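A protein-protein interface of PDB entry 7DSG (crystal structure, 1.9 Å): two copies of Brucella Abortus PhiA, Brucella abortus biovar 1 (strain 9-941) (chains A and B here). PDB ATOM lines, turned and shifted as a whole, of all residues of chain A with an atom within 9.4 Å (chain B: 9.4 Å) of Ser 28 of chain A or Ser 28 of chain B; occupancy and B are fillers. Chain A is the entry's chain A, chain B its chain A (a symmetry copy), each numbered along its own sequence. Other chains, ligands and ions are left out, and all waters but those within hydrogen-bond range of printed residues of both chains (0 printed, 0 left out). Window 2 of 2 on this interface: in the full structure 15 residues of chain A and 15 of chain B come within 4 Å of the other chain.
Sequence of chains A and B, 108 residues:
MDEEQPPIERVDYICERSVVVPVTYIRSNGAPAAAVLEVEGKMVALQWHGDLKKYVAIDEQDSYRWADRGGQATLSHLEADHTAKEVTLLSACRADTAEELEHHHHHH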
ATOM      1  N   PRO A   7      25.168  14.884  15.148  1.00  0.00           N
ATOM      2  CA  PRO A   7      25.580  16.284  15.103  1.00  0.00           C
ATOM      3  C   PRO A   7      26.389  16.608  16.347  1.00  0.00           C
ATOM      4  O   PRO A   7      26.053  16.167  17.448  1.00  0.00           O
ATOM      5  CB  PRO A   7      24.267  17.065  15.085  1.00  0.00           C
ATOM      6  CG  PRO A   7      23.191  16.049  14.774  1.00  0.00           C
ATOM      7  CD  PRO A   7      23.708  14.746  15.286  1.00  0.00           C
ATOM      8  N   ILE A   8      27.468  17.344  16.138  1.00  0.00           N
ATOM      9  CA  ILE A   8      28.352  17.790  17.204  1.00  0.00           C
ATOM     10  C   ILE A   8      28.426  19.302  17.122  1.00  0.00           C
ATOM     11  O   ILE A   8      28.707  19.855  16.053  1.00  0.00           O
ATOM     12  CB  ILE A   8      29.749  17.160  17.075  1.00  0.00           C
ATOM     13  CG1 ILE A   8      29.633  15.630  17.018  1.00  0.00           C
ATOM     14  CG2 ILE A   8      30.658  17.602  18.238  1.00  0.00           C
ATOM     15  CD1 ILE A   8      30.867  14.963  16.495  1.00  0.00           C
ATOM     16  N   TYR A  25      27.641  19.806  22.604  1.00  0.00           N
ATOM     17  CA  TYR A  25      26.387  19.074  22.498  1.00  0.00           C
ATOM     18  C   TYR A  25      26.523  18.006  21.434  1.00  0.00           C
ATOM     19  O   TYR A  25      27.025  18.278  20.338  1.00  0.00           O
ATOM     20  CB  TYR A  25      25.244  20.003  22.113  1.00  0.00           C
ATOM     21  CG  TYR A  25      24.831  20.953  23.203  1.00  0.00           C
ATOM     22  CD1 TYR A  25      24.243  20.491  24.369  1.00  0.00           C
ATOM     23  CD2 TYR A  25      24.992  22.311  23.043  1.00  0.00           C
ATOM     24  CE1 TYR A  25      23.845  21.365  25.345  1.00  0.00           C
ATOM     25  CE2 TYR A  25      24.600  23.182  24.011  1.00  0.00           C
ATOM     26  CZ  TYR A  25      24.034  22.715  25.158  1.00  0.00           C
ATOM     27  OH  TYR A  25      23.653  23.620  26.110  1.00  0.00           O
ATOM     28  N   ILE A  26      26.060  16.803  21.753  1.00  0.00           N
ATOM     29  CA  ILE A  26      26.020  15.693  20.815  1.00  0.00           C
ATOM     30  C   ILE A  26      24.555  15.308  20.680  1.00  0.00           C
ATOM     31  O   ILE A  26      23.880  15.052  21.685  1.00  0.00           O
ATOM     32  CB  ILE A  26      26.879  14.503  21.281  1.00  0.00           C
ATOM     33  CG1 ILE A  26      28.355  14.926  21.387  1.00  0.00           C
ATOM     34  CG2 ILE A  26      26.755  13.335  20.285  1.00  0.00           C
ATOM     35  CD1 ILE A  26      28.745  15.479  22.752  1.00  0.00           C
ATOM     36  N   ARG A  27      24.059  15.319  19.456  1.00  0.00           N
ATOM     37  CA  ARG A  27      22.685  14.937  19.178  1.00  0.00           C
ATOM     38  C   ARG A  27      22.689  13.593  18.473  1.00  0.00           C
ATOM     39  O   ARG A  27      23.693  13.179  17.894  1.00  0.00           O
ATOM     40  CB  ARG A  27      21.989  15.985  18.307  1.00  0.00           C
ATOM     41  CG  ARG A  27      21.810  17.319  19.002  1.00  0.00           C
ATOM     42  CD  ARG A  27      21.440  18.410  18.002  1.00  0.00           C
ATOM     43  NE  ARG A  27      20.101  18.209  17.459  1.00  0.00           N
ATOM     44  CZ  ARG A  27      18.981  18.307  18.171  1.00  0.00           C
ATOM     45  NH1 ARG A  27      19.031  18.610  19.464  1.00  0.00           N
ATOM     46  NH2 ARG A  27      17.809  18.103  17.585  1.00  0.00           N
ATOM     47  N   SER A  28      21.550  12.915  18.525  1.00  0.00           N
ATOM     48  CA  SER A  28      21.388  11.669  17.796  1.00  0.00           C
ATOM     49  C   SER A  28      19.981  11.669  17.225  1.00  0.00           C
ATOM     50  O   SER A  28      19.015  11.827  17.978  1.00  0.00           O
ATOM     51  CB  SER A  28      21.627  10.463  18.712  1.00  0.00           C
ATOM     52  OG  SER A  28      21.587   9.248  17.983  1.00  0.00           O
ATOM     53  N   ASN A  29      19.882  11.561  15.901  1.00  0.00           N
ATOM     54  CA  ASN A  29      18.612  11.478  15.171  1.00  0.00           C
ATOM     55  C   ASN A  29      17.606  12.507  15.683  1.00  0.00           C
ATOM     56  O   ASN A  29      16.525  12.186  16.177  1.00  0.00           O
ATOM     57  CB  ASN A  29      18.050  10.060  15.226  1.00  0.00           C
ATOM     58  CG  ASN A  29      18.974   9.063  14.560  1.00  0.00           C
ATOM     59  OD1 ASN A  29      19.441   9.303  13.451  1.00  0.00           O
ATOM     60  ND2 ASN A  29      19.302   7.982  15.260  1.00  0.00           N
ATOM     61  N   GLY A  30      18.010  13.771  15.574  1.00  0.00           N
ATOM     62  CA  GLY A  30      17.171  14.880  15.952  1.00  0.00           C
ATOM     63  C   GLY A  30      17.067  15.153  17.436  1.00  0.00           C
ATOM     64  O   GLY A  30      16.585  16.226  17.816  1.00  0.00           O
ATOM     65  N   ALA A  31      17.509  14.236  18.295  1.00  0.00           N
ATOM     66  CA  ALA A  31      17.207  14.473  19.691  1.00  0.00           C
ATOM     67  C   ALA A  31      18.482  14.782  20.474  1.00  0.00           C
ATOM     68  O   ALA A  31      19.568  14.332  20.093  1.00  0.00           O
ATOM     69  CB  ALA A  31      16.511  13.258  20.315  1.00  0.00           C
ATOM     70  N   PRO A  32      18.394  15.541  21.563  1.00  0.00           N
ATOM     71  CA  PRO A  32      19.576  15.691  22.424  1.00  0.00           C
ATOM     72  C   PRO A  32      19.977  14.324  22.955  1.00  0.00           C
ATOM     73  O   PRO A  32      19.129  13.466  23.205  1.00  0.00           O
ATOM     74  CB  PRO A  32      19.094  16.623  23.543  1.00  0.00           C
ATOM     75  CG  PRO A  32      17.877  17.304  22.997  1.00  0.00           C
ATOM     76  CD  PRO A  32      17.237  16.293  22.082  1.00  0.00           C
ATOM     77  N   ALA A  33      21.284  14.104  23.069  1.00  0.00           N
ATOM     78  CA  ALA A  33      21.768  12.854  23.641  1.00  0.00           C
ATOM     79  C   ALA A  33      22.780  13.114  24.749  1.00  0.00           C
ATOM     80  O   ALA A  33      22.641  12.615  25.868  1.00  0.00           O
ATOM     81  CB  ALA A  33      22.414  11.975  22.566  1.00  0.00           C
ATOM     82  N   ALA A  34      23.821  13.861  24.426  1.00  0.00           N
ATOM     83  CA  ALA A  34      24.913  14.061  25.362  1.00  0.00           C
ATOM     84  C   ALA A  34      25.320  15.518  25.367  1.00  0.00           C
ATOM     85  O   ALA A  34      25.142  16.241  24.379  1.00  0.00           O
ATOM     86  CB  ALA A  34      26.123  13.202  25.015  1.00  0.00           C
ATOM     87  N   TRP A  48      21.421  13.269  28.232  1.00  0.00           N
ATOM     88  CA  TRP A  48      20.098  13.865  28.198  1.00  0.00           C
ATOM     89  C   TRP A  48      19.106  12.972  28.928  1.00  0.00           C
ATOM     90  O   TRP A  48      19.107  11.751  28.767  1.00  0.00           O
ATOM     91  CB  TRP A  48      19.653  14.072  26.756  1.00  0.00           C
ATOM     92  CG  TRP A  48      18.259  14.576  26.618  1.00  0.00           C
ATOM     93  CD1 TRP A  48      17.186  13.899  26.101  1.00  0.00           C
ATOM     94  CD2 TRP A  48      17.778  15.874  26.976  1.00  0.00           C
ATOM     95  NE1 TRP A  48      16.070  14.699  26.121  1.00  0.00           N
ATOM     96  CE2 TRP A  48      16.406  15.918  26.649  1.00  0.00           C
ATOM     97  CE3 TRP A  48      18.374  17.009  27.535  1.00  0.00           C
ATOM     98  CZ2 TRP A  48      15.622  17.045  26.874  1.00  0.00           C
ATOM     99  CZ3 TRP A  48      17.596  18.128  27.757  1.00  0.00           C
ATOM    100  CH2 TRP A  48      16.232  18.136  27.430  1.00  0.00           C
ATOM    101  N   TYR A  55      20.147  17.635  31.092  1.00  0.00           N
ATOM    102  CA  TYR A  55      21.272  16.718  31.044  1.00  0.00           C
ATOM    103  C   TYR A  55      21.742  16.443  32.463  1.00  0.00           C
ATOM    104  O   TYR A  55      21.829  17.353  33.291  1.00  0.00           O
ATOM    105  CB  TYR A  55      22.424  17.294  30.226  1.00  0.00           C
ATOM    106  CG  TYR A  55      22.094  17.713  28.815  1.00  0.00           C
ATOM    107  CD1 TYR A  55      21.405  18.891  28.555  1.00  0.00           C
ATOM    108  CD2 TYR A  55      22.500  16.937  27.734  1.00  0.00           C
ATOM    109  CE1 TYR A  55      21.131  19.280  27.264  1.00  0.00           C
ATOM    110  CE2 TYR A  55      22.227  17.317  26.450  1.00  0.00           C
ATOM    111  CZ  TYR A  55      21.541  18.483  26.211  1.00  0.00           C
ATOM    112  OH  TYR A  55      21.281  18.843  24.905  1.00  0.00           O
ATOM    113  N   PRO B   7      25.981   5.604  24.114  1.00  0.00           N
ATOM    114  CA  PRO B   7      26.894   5.351  25.224  1.00  0.00           C
ATOM    115  C   PRO B   7      27.831   6.536  25.384  1.00  0.00           C
ATOM    116  O   PRO B   7      28.307   7.098  24.395  1.00  0.00           O
ATOM    117  CB  PRO B   7      27.662   4.099  24.803  1.00  0.00           C
ATOM    118  CG  PRO B   7      26.895   3.522  23.634  1.00  0.00           C
ATOM    119  CD  PRO B   7      26.214   4.683  22.989  1.00  0.00           C
ATOM    120  N   ILE B   8      28.046   6.917  26.631  1.00  0.00           N
ATOM    121  CA  ILE B   8      28.938   8.007  26.994  1.00  0.00           C
ATOM    122  C   ILE B   8      29.963   7.444  27.959  1.00  0.00           C
ATOM    123  O   ILE B   8      29.598   6.819  28.961  1.00  0.00           O
ATOM    124  CB  ILE B   8      28.167   9.178  27.625  1.00  0.00           C
ATOM    125  CG1 ILE B   8      27.043   9.636  26.686  1.00  0.00           C
ATOM    126  CG2 ILE B   8      29.118  10.344  27.958  1.00  0.00           C
ATOM    127  CD1 ILE B   8      26.007  10.474  27.367  1.00  0.00           C
ATOM    128  N   TYR B  25      34.139   9.871  25.202  1.00  0.00           N
ATOM    129  CA  TYR B  25      33.745   9.179  23.984  1.00  0.00           C
ATOM    130  C   TYR B  25      32.235   9.060  23.945  1.00  0.00           C
ATOM    131  O   TYR B  25      31.613   8.684  24.944  1.00  0.00           O
ATOM    132  CB  TYR B  25      34.344   7.780  23.933  1.00  0.00           C
ATOM    133  CG  TYR B  25      35.831   7.758  23.705  1.00  0.00           C
ATOM    134  CD1 TYR B  25      36.377   8.184  22.506  1.00  0.00           C
ATOM    135  CD2 TYR B  25      36.678   7.272  24.675  1.00  0.00           C
ATOM    136  CE1 TYR B  25      37.729   8.135  22.297  1.00  0.00           C
ATOM    137  CE2 TYR B  25      38.022   7.223  24.472  1.00  0.00           C
ATOM    138  CZ  TYR B  25      38.547   7.656  23.293  1.00  0.00           C
ATOM    139  OH  TYR B  25      39.904   7.592  23.125  1.00  0.00           O
ATOM    140  N   ILE B  26      31.658   9.363  22.789  1.00  0.00           N
ATOM    141  CA  ILE B  26      30.232   9.207  22.549  1.00  0.00           C
ATOM    142  C   ILE B  26      30.104   8.215  21.403  1.00  0.00           C
ATOM    143  O   ILE B  26      30.705   8.407  20.338  1.00  0.00           O
ATOM    144  CB  ILE B  26      29.545  10.545  22.220  1.00  0.00           C
ATOM    145  CG1 ILE B  26      29.679  11.514  23.409  1.00  0.00           C
ATOM    146  CG2 ILE B  26      28.052  10.316  21.917  1.00  0.00           C
ATOM    147  CD1 ILE B  26      30.931  12.381  23.364  1.00  0.00           C
ATOM    148  N   ARG B  27      29.371   7.142  21.639  1.00  0.00           N
ATOM    149  CA  ARG B  27      29.134   6.132  20.623  1.00  0.00           C
ATOM    150  C   ARG B  27      27.689   6.230  20.169  1.00  0.00           C
ATOM    151  O   ARG B  27      26.837   6.775  20.869  1.00  0.00           O
ATOM    152  CB  ARG B  27      29.421   4.730  21.164  1.00  0.00           C
ATOM    153  CG  ARG B  27      30.880   4.502  21.498  1.00  0.00           C
ATOM    154  CD  ARG B  27      31.057   3.245  22.343  1.00  0.00           C
ATOM    155  NE  ARG B  27      30.767   2.038  21.576  1.00  0.00           N
ATOM    156  CZ  ARG B  27      31.500   1.606  20.554  1.00  0.00           C
ATOM    157  NH1 ARG B  27      32.579   2.278  20.169  1.00  0.00           N
ATOM    158  NH2 ARG B  27      31.151   0.495  19.917  1.00  0.00           N
ATOM    159  N   SER B  28      27.422   5.692  18.986  1.00  0.00           N
ATOM    160  CA  SER B  28      26.058   5.621  18.489  1.00  0.00           C
ATOM    161  C   SER B  28      25.905   4.273  17.807  1.00  0.00           C
ATOM    162  O   SER B  28      26.684   3.953  16.903  1.00  0.00           O
ATOM    163  CB  SER B  28      25.763   6.778  17.528  1.00  0.00           C
ATOM    164  OG  SER B  28      24.402   6.782  17.131  1.00  0.00           O
ATOM    165  N   ASN B  29      24.954   3.473  18.287  1.00  0.00           N
ATOM    166  CA  ASN B  29      24.613   2.163  17.721  1.00  0.00           C
ATOM    167  C   ASN B  29      25.865   1.348  17.407  1.00  0.00           C
ATOM    168  O   ASN B  29      26.142   0.974  16.267  1.00  0.00           O
ATOM    169  CB  ASN B  29      23.717   2.322  16.495  1.00  0.00           C
ATOM    170  CG  ASN B  29      22.398   2.977  16.843  1.00  0.00           C
ATOM    171  OD1 ASN B  29      21.750   2.580  17.806  1.00  0.00           O
ATOM    172  ND2 ASN B  29      22.034   4.027  16.113  1.00  0.00           N
ATOM    173  N   GLY B  30      26.639   1.101  18.463  1.00  0.00           N
ATOM    174  CA  GLY B  30      27.831   0.297  18.369  1.00  0.00           C
ATOM    175  C   GLY B  30      29.042   0.981  17.775  1.00  0.00           C
ATOM    176  O   GLY B  30      30.153   0.450  17.899  1.00  0.00           O
ATOM    177  N   ALA B  31      28.884   2.144  17.144  1.00  0.00           N
ATOM    178  CA  ALA B  31      30.043   2.648  16.437  1.00  0.00           C
ATOM    179  C   ALA B  31      30.583   3.906  17.113  1.00  0.00           C
ATOM    180  O   ALA B  31      29.824   4.639  17.756  1.00  0.00           O
ATOM    181  CB  ALA B  31      29.699   2.963  14.977  1.00  0.00           C
ATOM    182  N   PRO B  32      31.877   4.190  16.993  1.00  0.00           N
ATOM    183  CA  PRO B  32      32.369   5.487  17.478  1.00  0.00           C
ATOM    184  C   PRO B  32      31.674   6.598  16.710  1.00  0.00           C
ATOM    185  O   PRO B  32      31.360   6.454  15.527  1.00  0.00           O
ATOM    186  CB  PRO B  32      33.874   5.438  17.181  1.00  0.00           C
ATOM    187  CG  PRO B  32      34.199   3.987  17.010  1.00  0.00           C
ATOM    188  CD  PRO B  32      32.959   3.373  16.413  1.00  0.00           C
ATOM    189  N   ALA B  33      31.376   7.692  17.407  1.00  0.00           N
ATOM    190  CA  ALA B  33      30.778   8.843  16.744  1.00  0.00           C
ATOM    191  C   ALA B  33      31.543  10.120  17.065  1.00  0.00           C
ATOM    192  O   ALA B  33      31.959  10.856  16.167  1.00  0.00           O
ATOM    193  CB  ALA B  33      29.315   9.016  17.162  1.00  0.00           C
ATOM    194  N   ALA B  34      31.696  10.404  18.347  1.00  0.00           N
ATOM    195  CA  ALA B  34      32.290  11.661  18.766  1.00  0.00           C
ATOM    196  C   ALA B  34      33.279  11.409  19.883  1.00  0.00           C
ATOM    197  O   ALA B  34      33.166  10.437  20.637  1.00  0.00           O
ATOM    198  CB  ALA B  34      31.237  12.657  19.239  1.00  0.00           C
ATOM    199  N   TRP B  48      34.219  11.102  14.640  1.00  0.00           N
ATOM    200  CA  TRP B  48      34.844   9.903  14.113  1.00  0.00           C
ATOM    201  C   TRP B  48      34.852   9.945  12.592  1.00  0.00           C
ATOM    202  O   TRP B  48      33.862  10.312  11.958  1.00  0.00           O
ATOM    203  CB  TRP B  48      34.098   8.667  14.598  1.00  0.00           C
ATOM    204  CG  TRP B  48      34.599   7.390  14.017  1.00  0.00           C
ATOM    205  CD1 TRP B  48      33.938   6.569  13.141  1.00  0.00           C
ATOM    206  CD2 TRP B  48      35.856   6.763  14.282  1.00  0.00           C
ATOM    207  NE1 TRP B  48      34.713   5.474  12.846  1.00  0.00           N
ATOM    208  CE2 TRP B  48      35.893   5.566  13.537  1.00  0.00           C
ATOM    209  CE3 TRP B  48      36.953   7.092  15.085  1.00  0.00           C
ATOM    210  CZ2 TRP B  48      36.986   4.706  13.561  1.00  0.00           C
ATOM    211  CZ3 TRP B  48      38.038   6.237  15.110  1.00  0.00           C
ATOM    212  CH2 TRP B  48      38.048   5.059  14.349  1.00  0.00           C
ATOM    213  N   TYR B  55      39.503  10.202  15.004  1.00  0.00           N
ATOM    214  CA  TYR B  55      38.624  11.331  15.249  1.00  0.00           C
ATOM    215  C   TYR B  55      39.301  12.598  14.752  1.00  0.00           C
ATOM    216  O   TYR B  55      40.501  12.799  14.958  1.00  0.00           O
ATOM    217  CB  TYR B  55      38.301  11.472  16.733  1.00  0.00           C
ATOM    218  CG  TYR B  55      37.710  10.257  17.404  1.00  0.00           C
ATOM    219  CD1 TYR B  55      38.499   9.166  17.744  1.00  0.00           C
ATOM    220  CD2 TYR B  55      36.357  10.214  17.723  1.00  0.00           C
ATOM    221  CE1 TYR B  55      37.958   8.072  18.380  1.00  0.00           C
ATOM    222  CE2 TYR B  55      35.814   9.129  18.351  1.00  0.00           C
ATOM    223  CZ  TYR B  55      36.608   8.056  18.678  1.00  0.00           C
ATOM    224  OH  TYR B  55      36.034   6.975  19.312  1.00  0.00           O
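N of Ala 33 of chain B lies within hydrogen-bond range of O of Ile 26 of chain B (3.1 Å). The backbone NH (N) of Ile 26 of chain A is in hydrogen-bond range of the backbone carbonyl oxygen (O) of Ala 34 of chain A, 2.8 Å away. O of Ile 26 of chain A lies within hydrogen-bond range of N of Ala 33 of chain A, 3.1 Å away. The backbone NH of Ile 26 of chain B lies within hydrogen-bond range of the backbone carbonyl oxygen of Ala 34 of chain B, at 2.8 Å.
Ile 8 of chain A touches Ala 34 of chain B. CG2 of Ile 26 of chain B touches CG2 of Ile 26 of chain A, 3.7 Å away. Ser 28 of chain A touches Ser 28 of chain B. Ala 34 of chain A touches Ile 8 of chain B.
Pro 7 of chain A touches none of the printed residues of chain B. Of the printed residues of chain B, Ile 8 of chain A touches Ala 34 (3.6 Å). Printed residues of chain B within 4 Å of Ile 26 of chain A: Ile 26 (3.7 Å). Of chain B, only Ser 28 (3.8 Å) comes within 4 Å of Ser 28 of chain A. No residue of chain B comes within 4 Å of Asn 29 of chain A. No residue of chain B comes within 4 Å of Ala 31 of chain A. Of the printed residues of chain B, Ala 34 of chain A touches Ile 8. Of the printed residues of chain A, Ile 26 of chain B touches Ile 26. Ser 28 of chain B touches just one residue of chain A: Ser 28 (3.8 Å). Asn 29 of chain B touches none of the printed residues of chain A. No residue of chain A comes within 4 Å of Gly 30 of chain B. No residue of chain A comes within 4 Å of Ala 31 of chain B. Pro 32 of chain B touches none of the printed residues of chain A. The nearest residue of chain B that does not touch Ser 28 of chain A is Asn 29 of chain B (5.6 Å). The nearest residue of chain A that does not touch Ser 28 of chain B is Asn 29 of chain A (5.6 Å).
Of the 14 printed residues of chain B, 4 touch a printed residue of chain A. Hydrophobic or aromatic side chains of chain B within 4 Å of the printed part of chain A: Ile 8, Ile 26 and Ala 34. Among the printed residues, 4 pairs touch across the chains.
Ile 8 of chain A touches Ala 34 of chain B, and with the chains exchanged Ala 34 of chain A touches Ile 8 of chain B. Ile 26 of chain A touches its own counterpart, Ile 26 of chain B. Ser 28 of chain A touches its own counterpart, Ser 28 of chain B. Positions printed for both chains: 7, 8, 25, 26, 27, 28, 29, 30, 31, 32, 33, 34, 48 and 55. Of the 4 pairs that touch across the chains among the printed residues, 4 have their exchanged pair printed and touching as well.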
